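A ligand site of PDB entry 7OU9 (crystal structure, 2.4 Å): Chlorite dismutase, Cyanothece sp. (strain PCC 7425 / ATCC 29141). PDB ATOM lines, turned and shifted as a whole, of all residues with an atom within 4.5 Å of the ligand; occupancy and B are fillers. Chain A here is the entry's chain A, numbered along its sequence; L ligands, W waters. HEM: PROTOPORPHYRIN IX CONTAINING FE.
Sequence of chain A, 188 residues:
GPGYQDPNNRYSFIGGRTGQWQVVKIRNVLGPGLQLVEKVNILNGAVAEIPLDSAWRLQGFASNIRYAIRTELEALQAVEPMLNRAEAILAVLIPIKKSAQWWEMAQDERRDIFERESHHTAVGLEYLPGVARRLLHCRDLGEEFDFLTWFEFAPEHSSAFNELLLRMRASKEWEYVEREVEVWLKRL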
ATOM      1  N   ASN A  64      15.642   5.822 -16.003  1.00  0.00           N
ATOM      2  CA  ASN A  64      16.842   5.841 -15.187  1.00  0.00           C
ATOM      3  C   ASN A  64      16.515   5.483 -13.736  1.00  0.00           C
ATOM      4  O   ASN A  64      15.363   5.491 -13.300  1.00  0.00           O
ATOM      5  CB  ASN A  64      17.498   7.224 -15.244  1.00  0.00           C
ATOM      6  CG  ASN A  64      16.560   8.323 -14.789  1.00  0.00           C
ATOM      7  OD1 ASN A  64      15.730   8.804 -15.564  1.00  0.00           O
ATOM      8  ND2 ASN A  64      16.680   8.731 -13.525  1.00  0.00           N
ATOM      9  N   ILE A  65      17.573   5.199 -12.973  1.00  0.00           N
ATOM     10  CA  ILE A  65      17.432   4.877 -11.566  1.00  0.00           C
ATOM     11  C   ILE A  65      16.932   6.100 -10.817  1.00  0.00           C
ATOM     12  O   ILE A  65      17.362   7.232 -11.074  1.00  0.00           O
ATOM     13  CB  ILE A  65      18.778   4.378 -11.000  1.00  0.00           C
ATOM     14  CG1 ILE A  65      19.096   2.969 -11.532  1.00  0.00           C
ATOM     15  CG2 ILE A  65      18.763   4.392  -9.477  1.00  0.00           C
ATOM     16  CD1 ILE A  65      18.105   1.891 -11.130  1.00  0.00           C
ATOM     17  N   ARG A  66      16.002   5.877  -9.873  1.00  0.00           N
ATOM     18  CA  ARG A  66      15.406   6.944  -9.082  1.00  0.00           C
ATOM     19  C   ARG A  66      15.718   6.882  -7.599  1.00  0.00           C
ATOM     20  O   ARG A  66      15.549   7.888  -6.911  1.00  0.00           O
ATOM     21  CB  ARG A  66      13.871   6.938  -9.247  1.00  0.00           C
ATOM     22  CG  ARG A  66      13.390   6.734 -10.677  1.00  0.00           C
ATOM     23  CD  ARG A  66      13.820   7.877 -11.572  1.00  0.00           C
ATOM     24  NE  ARG A  66      13.157   7.833 -12.867  1.00  0.00           N
ATOM     25  CZ  ARG A  66      11.954   8.331 -13.116  1.00  0.00           C
ATOM     26  NH1 ARG A  66      11.236   8.917 -12.177  1.00  0.00           N
ATOM     27  NH2 ARG A  66      11.459   8.229 -14.344  1.00  0.00           N
ATOM     28  N   TYR A  67      16.166   5.737  -7.087  1.00  0.00           N
ATOM     29  CA  TYR A  67      16.404   5.573  -5.653  1.00  0.00           C
ATOM     30  C   TYR A  67      17.669   4.777  -5.369  1.00  0.00           C
ATOM     31  O   TYR A  67      18.410   5.098  -4.436  1.00  0.00           O
ATOM     32  CB  TYR A  67      15.202   4.873  -4.999  1.00  0.00           C
ATOM     33  CG  TYR A  67      13.905   5.661  -5.101  1.00  0.00           C
ATOM     34  CD1 TYR A  67      13.705   6.793  -4.332  1.00  0.00           C
ATOM     35  CD2 TYR A  67      12.892   5.257  -5.956  1.00  0.00           C
ATOM     36  CE1 TYR A  67      12.524   7.510  -4.415  1.00  0.00           C
ATOM     37  CE2 TYR A  67      11.709   5.964  -6.048  1.00  0.00           C
ATOM     38  CZ  TYR A  67      11.531   7.086  -5.273  1.00  0.00           C
ATOM     39  OH  TYR A  67      10.360   7.804  -5.358  1.00  0.00           O
ATOM     40  N   ALA A  68      17.918   3.734  -6.154  1.00  0.00           N
ATOM     41  CA  ALA A  68      19.016   2.828  -5.877  1.00  0.00           C
ATOM     42  C   ALA A  68      20.342   3.572  -5.801  1.00  0.00           C
ATOM     43  O   ALA A  68      20.640   4.450  -6.620  1.00  0.00           O
ATOM     44  CB  ALA A  68      19.097   1.739  -6.950  1.00  0.00           C
ATOM     45  N   LEU A  76      23.132  -5.672  -6.921  1.00  0.00           N
ATOM     46  CA  LEU A  76      22.173  -6.271  -7.838  1.00  0.00           C
ATOM     47  C   LEU A  76      22.860  -6.767  -9.105  1.00  0.00           C
ATOM     48  O   LEU A  76      22.608  -7.884  -9.557  1.00  0.00           O
ATOM     49  CB  LEU A  76      21.073  -5.250  -8.184  1.00  0.00           C
ATOM     50  CG  LEU A  76      20.319  -4.648  -7.001  1.00  0.00           C
ATOM     51  CD1 LEU A  76      20.085  -3.165  -7.190  1.00  0.00           C
ATOM     52  CD2 LEU A  76      18.986  -5.354  -6.789  1.00  0.00           C
ATOM     53  N   ILE A  94       2.725  -7.068 -12.598  1.00  0.00           N
ATOM     54  CA  ILE A  94       2.018  -6.441 -11.479  1.00  0.00           C
ATOM     55  C   ILE A  94       1.963  -4.932 -11.700  1.00  0.00           C
ATOM     56  O   ILE A  94       2.891  -4.214 -11.296  1.00  0.00           O
ATOM     57  CB  ILE A  94       2.681  -6.786 -10.140  1.00  0.00           C
ATOM     58  CG1 ILE A  94       2.967  -8.285 -10.034  1.00  0.00           C
ATOM     59  CG2 ILE A  94       1.814  -6.325  -8.985  1.00  0.00           C
ATOM     60  CD1 ILE A  94       3.660  -8.693  -8.739  1.00  0.00           C
ATOM     61  N   ILE A  96       0.985  -1.243 -10.692  1.00  0.00           N
ATOM     62  CA  ILE A  96       0.866  -0.609  -9.377  1.00  0.00           C
ATOM     63  C   ILE A  96       0.572   0.875  -9.563  1.00  0.00           C
ATOM     64  O   ILE A  96       1.112   1.516 -10.464  1.00  0.00           O
ATOM     65  CB  ILE A  96       2.148  -0.800  -8.537  1.00  0.00           C
ATOM     66  CG1 ILE A  96       2.202  -2.209  -7.972  1.00  0.00           C
ATOM     67  CG2 ILE A  96       2.194   0.202  -7.395  1.00  0.00           C
ATOM     68  CD1 ILE A  96       3.605  -2.757  -7.878  1.00  0.00           C
ATOM     69  N   LYS A  98       0.425   4.365  -6.944  1.00  0.00           N
ATOM     70  CA  LYS A  98       0.684   4.915  -5.628  1.00  0.00           C
ATOM     71  C   LYS A  98      -0.160   6.169  -5.409  1.00  0.00           C
ATOM     72  O   LYS A  98      -0.533   6.855  -6.361  1.00  0.00           O
ATOM     73  CB  LYS A  98       2.169   5.223  -5.440  1.00  0.00           C
ATOM     74  CG  LYS A  98       2.962   4.001  -4.982  1.00  0.00           C
ATOM     75  CD  LYS A  98       4.437   4.299  -4.790  1.00  0.00           C
ATOM     76  CE  LYS A  98       5.263   3.014  -4.860  1.00  0.00           C
ATOM     77  NZ  LYS A  98       6.684   3.206  -4.444  1.00  0.00           N
ATOM     78  N   TRP A 102       1.996  10.022  -1.896  1.00  0.00           N
ATOM     79  CA  TRP A 102       3.361   9.572  -2.159  1.00  0.00           C
ATOM     80  C   TRP A 102       4.070  10.518  -3.116  1.00  0.00           C
ATOM     81  O   TRP A 102       5.228  10.892  -2.887  1.00  0.00           O
ATOM     82  CB  TRP A 102       3.323   8.155  -2.723  1.00  0.00           C
ATOM     83  CG  TRP A 102       4.624   7.684  -3.319  1.00  0.00           C
ATOM     84  CD1 TRP A 102       4.974   7.720  -4.633  1.00  0.00           C
ATOM     85  CD2 TRP A 102       5.731   7.106  -2.622  1.00  0.00           C
ATOM     86  NE1 TRP A 102       6.237   7.197  -4.797  1.00  0.00           N
ATOM     87  CE2 TRP A 102       6.718   6.807  -3.578  1.00  0.00           C
ATOM     88  CE3 TRP A 102       5.977   6.796  -1.272  1.00  0.00           C
ATOM     89  CZ2 TRP A 102       7.941   6.235  -3.236  1.00  0.00           C
ATOM     90  CZ3 TRP A 102       7.188   6.224  -0.938  1.00  0.00           C
ATOM     91  CH2 TRP A 102       8.161   5.944  -1.913  1.00  0.00           C
ATOM     92  N   PHE A 114      11.266   4.037   0.958  1.00  0.00           N
ATOM     93  CA  PHE A 114      11.530   2.954   0.017  1.00  0.00           C
ATOM     94  C   PHE A 114      12.543   1.967   0.565  1.00  0.00           C
ATOM     95  O   PHE A 114      12.364   0.748   0.442  1.00  0.00           O
ATOM     96  CB  PHE A 114      12.002   3.539  -1.317  1.00  0.00           C
ATOM     97  CG  PHE A 114      12.330   2.510  -2.347  1.00  0.00           C
ATOM     98  CD1 PHE A 114      11.328   1.856  -3.035  1.00  0.00           C
ATOM     99  CD2 PHE A 114      13.649   2.198  -2.648  1.00  0.00           C
ATOM    100  CE1 PHE A 114      11.621   0.902  -4.000  1.00  0.00           C
ATOM    101  CE2 PHE A 114      13.954   1.254  -3.606  1.00  0.00           C
ATOM    102  CZ  PHE A 114      12.945   0.611  -4.284  1.00  0.00           C
ATOM    103  N   HIS A 120      13.255  -2.278   0.574  1.00  0.00           N
ATOM    104  CA  HIS A 120      12.784  -2.862  -0.681  1.00  0.00           C
ATOM    105  C   HIS A 120      13.888  -3.628  -1.389  1.00  0.00           C
ATOM    106  O   HIS A 120      13.694  -4.774  -1.811  1.00  0.00           O
ATOM    107  CB  HIS A 120      12.219  -1.750  -1.574  1.00  0.00           C
ATOM    108  CG  HIS A 120      11.640  -2.244  -2.862  1.00  0.00           C
ATOM    109  ND1 HIS A 120      10.282  -2.256  -3.107  1.00  0.00           N
ATOM    110  CD2 HIS A 120      12.228  -2.740  -3.973  1.00  0.00           C
ATOM    111  CE1 HIS A 120      10.068  -2.730  -4.325  1.00  0.00           C
ATOM    112  NE2 HIS A 120      11.230  -3.036  -4.868  1.00  0.00           N
ATOM    113  N   THR A 121      15.062  -3.016  -1.518  1.00  0.00           N
ATOM    114  CA  THR A 121      16.135  -3.625  -2.290  1.00  0.00           C
ATOM    115  C   THR A 121      16.814  -4.757  -1.525  1.00  0.00           C
ATOM    116  O   THR A 121      17.120  -5.808  -2.106  1.00  0.00           O
ATOM    117  CB  THR A 121      17.157  -2.558  -2.689  1.00  0.00           C
ATOM    118  OG1 THR A 121      16.537  -1.615  -3.580  1.00  0.00           O
ATOM    119  CG2 THR A 121      18.361  -3.183  -3.377  1.00  0.00           C
ATOM    120  N   GLY A 124      14.402  -7.585  -1.784  1.00  0.00           N
ATOM    121  CA  GLY A 124      14.361  -8.119  -3.140  1.00  0.00           C
ATOM    122  C   GLY A 124      15.612  -8.896  -3.511  1.00  0.00           C
ATOM    123  O   GLY A 124      15.539  -9.864  -4.279  1.00  0.00           O
ATOM    124  N   LEU A 125      16.768  -8.493  -2.976  1.00  0.00           N
ATOM    125  CA  LEU A 125      18.014  -9.186  -3.289  1.00  0.00           C
ATOM    126  C   LEU A 125      18.024 -10.617  -2.775  1.00  0.00           C
ATOM    127  O   LEU A 125      18.755 -11.449  -3.312  1.00  0.00           O
ATOM    128  CB  LEU A 125      19.198  -8.420  -2.710  1.00  0.00           C
ATOM    129  CG  LEU A 125      19.946  -7.547  -3.713  1.00  0.00           C
ATOM    130  CD1 LEU A 125      20.737  -6.469  -3.002  1.00  0.00           C
ATOM    131  CD2 LEU A 125      20.859  -8.401  -4.578  1.00  0.00           C
ATOM    132  N   LEU A 128      17.110 -13.267  -5.594  1.00  0.00           N
ATOM    133  CA  LEU A 128      17.948 -13.398  -6.773  1.00  0.00           C
ATOM    134  C   LEU A 128      18.990 -14.496  -6.543  1.00  0.00           C
ATOM    135  O   LEU A 128      19.423 -14.721  -5.416  1.00  0.00           O
ATOM    136  CB  LEU A 128      18.663 -12.083  -7.106  1.00  0.00           C
ATOM    137  CG  LEU A 128      17.835 -11.051  -7.883  1.00  0.00           C
ATOM    138  CD1 LEU A 128      16.428 -10.942  -7.313  1.00  0.00           C
ATOM    139  CD2 LEU A 128      18.514  -9.695  -7.882  1.00  0.00           C
ATOM    140  N   VAL A 131      14.716 -14.838  -9.496  1.00  0.00           N
ATOM    141  CA  VAL A 131      13.698 -13.983 -10.097  1.00  0.00           C
ATOM    142  C   VAL A 131      14.381 -12.931 -10.952  1.00  0.00           C
ATOM    143  O   VAL A 131      15.220 -12.166 -10.448  1.00  0.00           O
ATOM    144  CB  VAL A 131      12.806 -13.328  -9.030  1.00  0.00           C
ATOM    145  CG1 VAL A 131      11.630 -12.625  -9.678  1.00  0.00           C
ATOM    146  CG2 VAL A 131      12.321 -14.373  -8.025  1.00  0.00           C
ATOM    147  N   ARG A 133      13.654  -9.460 -13.264  1.00  0.00           N
ATOM    148  CA  ARG A 133      12.703  -8.368 -13.092  1.00  0.00           C
ATOM    149  C   ARG A 133      12.973  -7.260 -14.103  1.00  0.00           C
ATOM    150  O   ARG A 133      14.097  -7.101 -14.594  1.00  0.00           O
ATOM    151  CB  ARG A 133      12.749  -7.780 -11.679  1.00  0.00           C
ATOM    152  CG  ARG A 133      14.161  -7.425 -11.230  1.00  0.00           C
ATOM    153  CD  ARG A 133      14.160  -6.779  -9.851  1.00  0.00           C
ATOM    154  NE  ARG A 133      13.636  -5.414  -9.906  1.00  0.00           N
ATOM    155  CZ  ARG A 133      14.370  -4.333 -10.127  1.00  0.00           C
ATOM    156  NH1 ARG A 133      15.676  -4.405 -10.285  1.00  0.00           N
ATOM    157  NH2 ARG A 133      13.770  -3.138 -10.185  1.00  0.00           N
ATOM    158  N   LEU A 135      11.442  -3.112 -14.506  1.00  0.00           N
ATOM    159  CA  LEU A 135      10.614  -2.049 -13.970  1.00  0.00           C
ATOM    160  C   LEU A 135      10.327  -1.033 -15.075  1.00  0.00           C
ATOM    161  O   LEU A 135      11.255  -0.499 -15.698  1.00  0.00           O
ATOM    162  CB  LEU A 135      11.289  -1.371 -12.777  1.00  0.00           C
ATOM    163  CG  LEU A 135      10.542  -0.184 -12.165  1.00  0.00           C
ATOM    164  CD1 LEU A 135       9.334  -0.674 -11.379  1.00  0.00           C
ATOM    165  CD2 LEU A 135      11.476   0.633 -11.296  1.00  0.00           C
ATOM    166  N   PHE A 147       3.208   2.241 -12.339  1.00  0.00           N
ATOM    167  CA  PHE A 147       4.303   1.356 -12.709  1.00  0.00           C
ATOM    168  C   PHE A 147       3.736   0.081 -13.316  1.00  0.00           C
ATOM    169  O   PHE A 147       2.617  -0.339 -13.006  1.00  0.00           O
ATOM    170  CB  PHE A 147       5.190   0.990 -11.513  1.00  0.00           C
ATOM    171  CG  PHE A 147       5.665   2.167 -10.715  1.00  0.00           C
ATOM    172  CD1 PHE A 147       6.769   2.893 -11.122  1.00  0.00           C
ATOM    173  CD2 PHE A 147       5.001   2.546  -9.559  1.00  0.00           C
ATOM    174  CE1 PHE A 147       7.208   3.977 -10.382  1.00  0.00           C
ATOM    175  CE2 PHE A 147       5.440   3.619  -8.819  1.00  0.00           C
ATOM    176  CZ  PHE A 147       6.544   4.345  -9.226  1.00  0.00           C
ATOM    177  N   THR A 149       5.399  -3.554 -13.200  1.00  0.00           N
ATOM    178  CA  THR A 149       6.494  -4.410 -12.760  1.00  0.00           C
ATOM    179  C   THR A 149       6.352  -5.772 -13.428  1.00  0.00           C
ATOM    180  O   THR A 149       5.237  -6.255 -13.639  1.00  0.00           O
ATOM    181  CB  THR A 149       6.524  -4.567 -11.248  1.00  0.00           C
ATOM    182  OG1 THR A 149       5.298  -5.159 -10.801  1.00  0.00           O
ATOM    183  CG2 THR A 149       6.687  -3.214 -10.575  1.00  0.00           C
ATOM    184  N   PHE A 151       8.102  -9.783 -13.524  1.00  0.00           N
ATOM    185  CA  PHE A 151       8.958 -10.774 -12.899  1.00  0.00           C
ATOM    186  C   PHE A 151       8.772 -12.090 -13.631  1.00  0.00           C
ATOM    187  O   PHE A 151       7.660 -12.417 -14.068  1.00  0.00           O
ATOM    188  CB  PHE A 151       8.622 -10.930 -11.417  1.00  0.00           C
ATOM    189  CG  PHE A 151       8.553  -9.621 -10.678  1.00  0.00           C
ATOM    190  CD1 PHE A 151       9.706  -9.050 -10.173  1.00  0.00           C
ATOM    191  CD2 PHE A 151       7.359  -8.950 -10.539  1.00  0.00           C
ATOM    192  CE1 PHE A 151       9.657  -7.847  -9.514  1.00  0.00           C
ATOM    193  CE2 PHE A 151       7.299  -7.747  -9.889  1.00  0.00           C
ATOM    194  CZ  PHE A 151       8.452  -7.186  -9.383  1.00  0.00           C
ATOM    195  N   PHE A 161       8.453 -16.546  -4.716  1.00  0.00           N
ATOM    196  CA  PHE A 161       7.924 -15.278  -5.195  1.00  0.00           C
ATOM    197  C   PHE A 161       6.696 -14.857  -4.408  1.00  0.00           C
ATOM    198  O   PHE A 161       6.550 -13.681  -4.044  1.00  0.00           O
ATOM    199  CB  PHE A 161       7.585 -15.367  -6.685  1.00  0.00           C
ATOM    200  CG  PHE A 161       7.144 -14.057  -7.279  1.00  0.00           C
ATOM    201  CD1 PHE A 161       8.052 -13.024  -7.454  1.00  0.00           C
ATOM    202  CD2 PHE A 161       5.827 -13.846  -7.640  1.00  0.00           C
ATOM    203  CE1 PHE A 161       7.652 -11.811  -7.991  1.00  0.00           C
ATOM    204  CE2 PHE A 161       5.417 -12.632  -8.174  1.00  0.00           C
ATOM    205  CZ  PHE A 161       6.334 -11.610  -8.351  1.00  0.00           C
ATOM    206  N   LEU A 164       7.653 -13.427  -1.228  1.00  0.00           N
ATOM    207  CA  LEU A 164       8.144 -12.061  -1.421  1.00  0.00           C
ATOM    208  C   LEU A 164       6.988 -11.066  -1.557  1.00  0.00           C
ATOM    209  O   LEU A 164       7.074  -9.935  -1.069  1.00  0.00           O
ATOM    210  CB  LEU A 164       9.046 -11.996  -2.657  1.00  0.00           C
ATOM    211  CG  LEU A 164       9.343 -10.613  -3.259  1.00  0.00           C
ATOM    212  CD1 LEU A 164      10.263  -9.795  -2.356  1.00  0.00           C
ATOM    213  CD2 LEU A 164       9.962 -10.764  -4.633  1.00  0.00           C
ATOM    214  N   LEU A 165       5.896 -11.477  -2.219  1.00  0.00           N
ATOM    215  CA  LEU A 165       4.739 -10.602  -2.347  1.00  0.00           C
ATOM    216  C   LEU A 165       4.175 -10.232  -0.978  1.00  0.00           C
ATOM    217  O   LEU A 165       3.909  -9.059  -0.690  1.00  0.00           O
ATOM    218  CB  LEU A 165       3.659 -11.266  -3.203  1.00  0.00           C
ATOM    219  CG  LEU A 165       3.933 -11.332  -4.709  1.00  0.00           C
ATOM    220  CD1 LEU A 165       2.874 -12.176  -5.405  1.00  0.00           C
ATOM    221  CD2 LEU A 165       3.994  -9.937  -5.310  1.00  0.00           C
ATOM    222  N   MET A 168       6.592  -7.774   0.751  1.00  0.00           N
ATOM    223  CA  MET A 168       6.511  -6.424   0.206  1.00  0.00           C
ATOM    224  C   MET A 168       5.236  -5.732   0.660  1.00  0.00           C
ATOM    225  O   MET A 168       5.250  -4.539   1.007  1.00  0.00           O
ATOM    226  CB  MET A 168       6.577  -6.468  -1.316  1.00  0.00           C
ATOM    227  CG  MET A 168       7.958  -6.808  -1.887  1.00  0.00           C
ATOM    228  SD  MET A 168       9.026  -5.364  -2.031  1.00  0.00           S
ATOM    229  CE  MET A 168      10.576  -6.032  -1.408  1.00  0.00           C
ATOM    230  N   GLU A 173       6.094   1.038   2.527  1.00  0.00           N
ATOM    231  CA  GLU A 173       5.937   1.495   1.148  1.00  0.00           C
ATOM    232  C   GLU A 173       4.546   1.155   0.611  1.00  0.00           C
ATOM    233  O   GLU A 173       3.928   1.970  -0.078  1.00  0.00           O
ATOM    234  CB  GLU A 173       7.024   0.889   0.259  1.00  0.00           C
ATOM    235  CG  GLU A 173       6.827   1.109  -1.229  1.00  0.00           C
ATOM    236  CD  GLU A 173       7.967   0.555  -2.071  1.00  0.00           C
ATOM    237  OE1 GLU A 173       8.766  -0.241  -1.538  1.00  0.00           O
ATOM    238  OE2 GLU A 173       8.065   0.921  -3.266  1.00  0.00           O
ATOM    239  N   TRP A 174       4.047  -0.033   0.929  1.00  0.00           N
ATOM    240  CA  TRP A 174       2.772  -0.476   0.372  1.00  0.00           C
ATOM    241  C   TRP A 174       1.569   0.187   1.016  1.00  0.00           C
ATOM    242  O   TRP A 174       0.454   0.045   0.497  1.00  0.00           O
ATOM    243  CB  TRP A 174       2.648  -2.001   0.481  1.00  0.00           C
ATOM    244  CG  TRP A 174       2.433  -2.643  -0.860  1.00  0.00           C
ATOM    245  CD1 TRP A 174       1.256  -3.132  -1.344  1.00  0.00           C
ATOM    246  CD2 TRP A 174       3.408  -2.856  -1.880  1.00  0.00           C
ATOM    247  NE1 TRP A 174       1.440  -3.643  -2.609  1.00  0.00           N
ATOM    248  CE2 TRP A 174       2.759  -3.487  -2.959  1.00  0.00           C
ATOM    249  CE3 TRP A 174       4.775  -2.584  -1.981  1.00  0.00           C
ATOM    250  CZ2 TRP A 174       3.431  -3.836  -4.128  1.00  0.00           C
ATOM    251  CZ3 TRP A 174       5.437  -2.934  -3.148  1.00  0.00           C
ATOM    252  CH2 TRP A 174       4.764  -3.563  -4.201  1.00  0.00           C
ATOM    253  N   GLU A 180      -3.512  -2.381  -7.281  1.00  0.00           N
ATOM    254  CA  GLU A 180      -2.580  -3.461  -7.582  1.00  0.00           C
ATOM    255  C   GLU A 180      -3.339  -4.606  -8.235  1.00  0.00           C
ATOM    256  O   GLU A 180      -4.441  -4.950  -7.811  1.00  0.00           O
ATOM    257  CB  GLU A 180      -1.875  -3.950  -6.316  1.00  0.00           C
ATOM    258  CG  GLU A 180      -0.533  -4.620  -6.571  1.00  0.00           C
ATOM    259  CD  GLU A 180       0.135  -5.079  -5.288  1.00  0.00           C
ATOM    260  OE1 GLU A 180      -0.153  -4.489  -4.220  1.00  0.00           O
ATOM    261  OE2 GLU A 180       0.983  -6.002  -5.343  1.00  0.00           O
HETATM  262  CHA HEM L   1      11.624  -0.235  -7.641  1.00  0.00           C
HETATM  263  CHB HEM L   1      14.506  -4.022  -6.694  1.00  0.00           C
HETATM  264  CHC HEM L   1      10.633  -6.915  -6.289  1.00  0.00           C
HETATM  265  CHD HEM L   1       7.738  -3.111  -7.111  1.00  0.00           C
HETATM  266  C1A HEM L   1      12.740  -1.002  -7.387  1.00  0.00           C
HETATM  267  C2A HEM L   1      14.115  -0.518  -7.296  1.00  0.00           C
HETATM  268  C3A HEM L   1      14.898  -1.572  -7.032  1.00  0.00           C
HETATM  269  C4A HEM L   1      14.067  -2.751  -6.957  1.00  0.00           C
HETATM  270  CMA HEM L   1      16.425  -1.536  -6.857  1.00  0.00           C
HETATM  271  CAA HEM L   1      14.596   0.930  -7.451  1.00  0.00           C
HETATM  272  CBA HEM L   1      14.482   1.372  -8.910  1.00  0.00           C
HETATM  273  CGA HEM L   1      15.040   2.772  -9.038  1.00  0.00           C
HETATM  274  O1A HEM L   1      15.920   3.174  -8.225  1.00  0.00           O
HETATM  275  O2A HEM L   1      14.599   3.489  -9.977  1.00  0.00           O
HETATM  276  C1B HEM L   1      13.706  -5.139  -6.579  1.00  0.00           C
HETATM  277  C2B HEM L   1      14.191  -6.503  -6.515  1.00  0.00           C
HETATM  278  C3B HEM L   1      13.136  -7.308  -6.423  1.00  0.00           C
HETATM  279  C4B HEM L   1      11.942  -6.484  -6.396  1.00  0.00           C
HETATM  280  CMB HEM L   1      15.671  -6.922  -6.590  1.00  0.00           C
HETATM  281  CAB HEM L   1      13.221  -8.857  -6.340  1.00  0.00           C
HETATM  282  CBB HEM L   1      12.202  -9.623  -6.730  1.00  0.00           C
HETATM  283  C1C HEM L   1       9.508  -6.133  -6.450  1.00  0.00           C
HETATM  284  C2C HEM L   1       8.133  -6.595  -6.357  1.00  0.00           C
HETATM  285  C3C HEM L   1       7.335  -5.550  -6.597  1.00  0.00           C
HETATM  286  C4C HEM L   1       8.179  -4.390  -6.837  1.00  0.00           C
HETATM  287  CMC HEM L   1       7.717  -8.055  -6.052  1.00  0.00           C
HETATM  288  CAC HEM L   1       5.795  -5.486  -6.611  1.00  0.00           C
HETATM  289  CBC HEM L   1       5.021  -6.450  -6.121  1.00  0.00           C
HETATM  290  C1D HEM L   1       8.523  -2.010  -7.335  1.00  0.00           C
HETATM  291  C2D HEM L   1       8.063  -0.682  -7.648  1.00  0.00           C
HETATM  292  C3D HEM L   1       9.136   0.110  -7.795  1.00  0.00           C
HETATM  293  C4D HEM L   1      10.316  -0.689  -7.574  1.00  0.00           C
HETATM  294  CMD HEM L   1       6.578  -0.265  -7.778  1.00  0.00           C
HETATM  295  CAD HEM L   1       9.127   1.612  -8.129  1.00  0.00           C
HETATM  296  CBD HEM L   1       8.922   2.415  -6.847  1.00  0.00           C
HETATM  297  CGD HEM L   1       9.004   3.889  -7.138  1.00  0.00           C
HETATM  298  O1D HEM L   1       9.783   4.296  -8.048  1.00  0.00           O
HETATM  299  O2D HEM L   1       8.299   4.661  -6.439  1.00  0.00           O
HETATM  300  NA  HEM L   1      12.755  -2.361  -7.176  1.00  0.00           N
HETATM  301  NB  HEM L   1      12.328  -5.171  -6.500  1.00  0.00           N
HETATM  302  NC  HEM L   1       9.494  -4.788  -6.742  1.00  0.00           N
HETATM  303  ND  HEM L   1       9.906  -1.981  -7.301  1.00  0.00           N
HETATM  304 FE   HEM L   1      11.124  -3.562  -6.919  1.00  0.00          FE
HETATM  305  O   HOH W   1       9.530   6.894  -9.347  1.00  0.00           O
HETATM  306  O   HOH W   2      13.884   3.197 -12.386  1.00  0.00           O
HETATM  307  O   HOH W   3      11.975   3.443  -9.512  1.00  0.00           O
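Water W2 lies within hydrogen-bond range of an oxygen (O2A) of the ligand (2.5 Å) and the backbone carbonyl oxygen (O) of Asn 64 (2.9 Å).
The backbone NH (N) of His 120 lies within hydrogen-bond range of the backbone carbonyl oxygen (O) of Phe 114 (3.2 Å). OE1 of Glu 173 is in hydrogen-bond range of ND1 of His 120. ND1 of His 120 lies within hydrogen-bond range of SD of Met 168. The guanidinium group of Arg 66 sits at hydrogen-bond distance from the backbone carbonyl oxygen of Asn 64 (3.2 Å). OE2 of Glu 173 is in salt-bridge range of NZ of Lys 98, 2.9 Å away. NE1 of Trp 174 sits at hydrogen-bond distance from OE1 of Glu 180 (2.4 Å). The backbone NH (N) of Phe 147 lies within hydrogen-bond range of the backbone carbonyl oxygen (O) of Ile 96, 2.9 Å away. The side-chain hydroxyl (OG1) of Thr 149 is in hydrogen-bond range of the backbone carbonyl oxygen (O) of Ile 94, 2.6 Å away.
The guanidinium group (NH2) of Arg 133 lies close to a nitrogen (NA) of the ligand (3.3 Å). Merely in contact with the ligand: Phe 151 (3.1 Å), Trp 174 (3.3 Å), Phe 147 (3.3 Å), Gly 124 (3.3 Å), Leu 164 (3.3 Å), Thr 121 (3.3 Å), Ile 65 (3.3 Å), Phe 114 (3.4 Å), Trp 102 (3.6 Å), Thr 149 (3.6 Å), Leu 76 (3.7 Å), Leu 135 (3.7 Å), Ile 94 (3.7 Å), Ile 96 (3.7 Å), Leu 165 (3.7 Å), Leu 128 (3.9 Å), Asn 64 (3.95 Å) and Glu 173 (3.97 Å). The nearest printed residue that does not touch the ligand is Leu 125 (4.1 Å).
A ring nitrogen (NE2) of His 120 binds an iron atom (FE) of the ligand (2.1 Å). The backbone NH (N) of Arg 66 is in hydrogen-bond range of an oxygen (O2A) of the ligand, 2.8 Å away. The backbone NH (N) of Tyr 67 sits at hydrogen-bond distance from an oxygen (O1A) of the ligand (2.8 Å). An oxygen (O1A) of the ligand sits at hydrogen-bond distance from the backbone NH of Ala 68, 2.9 Å away. An oxygen (O2D) of the ligand lies within salt-bridge range of the side-chain amino group of Lys 98 (3.0 Å).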
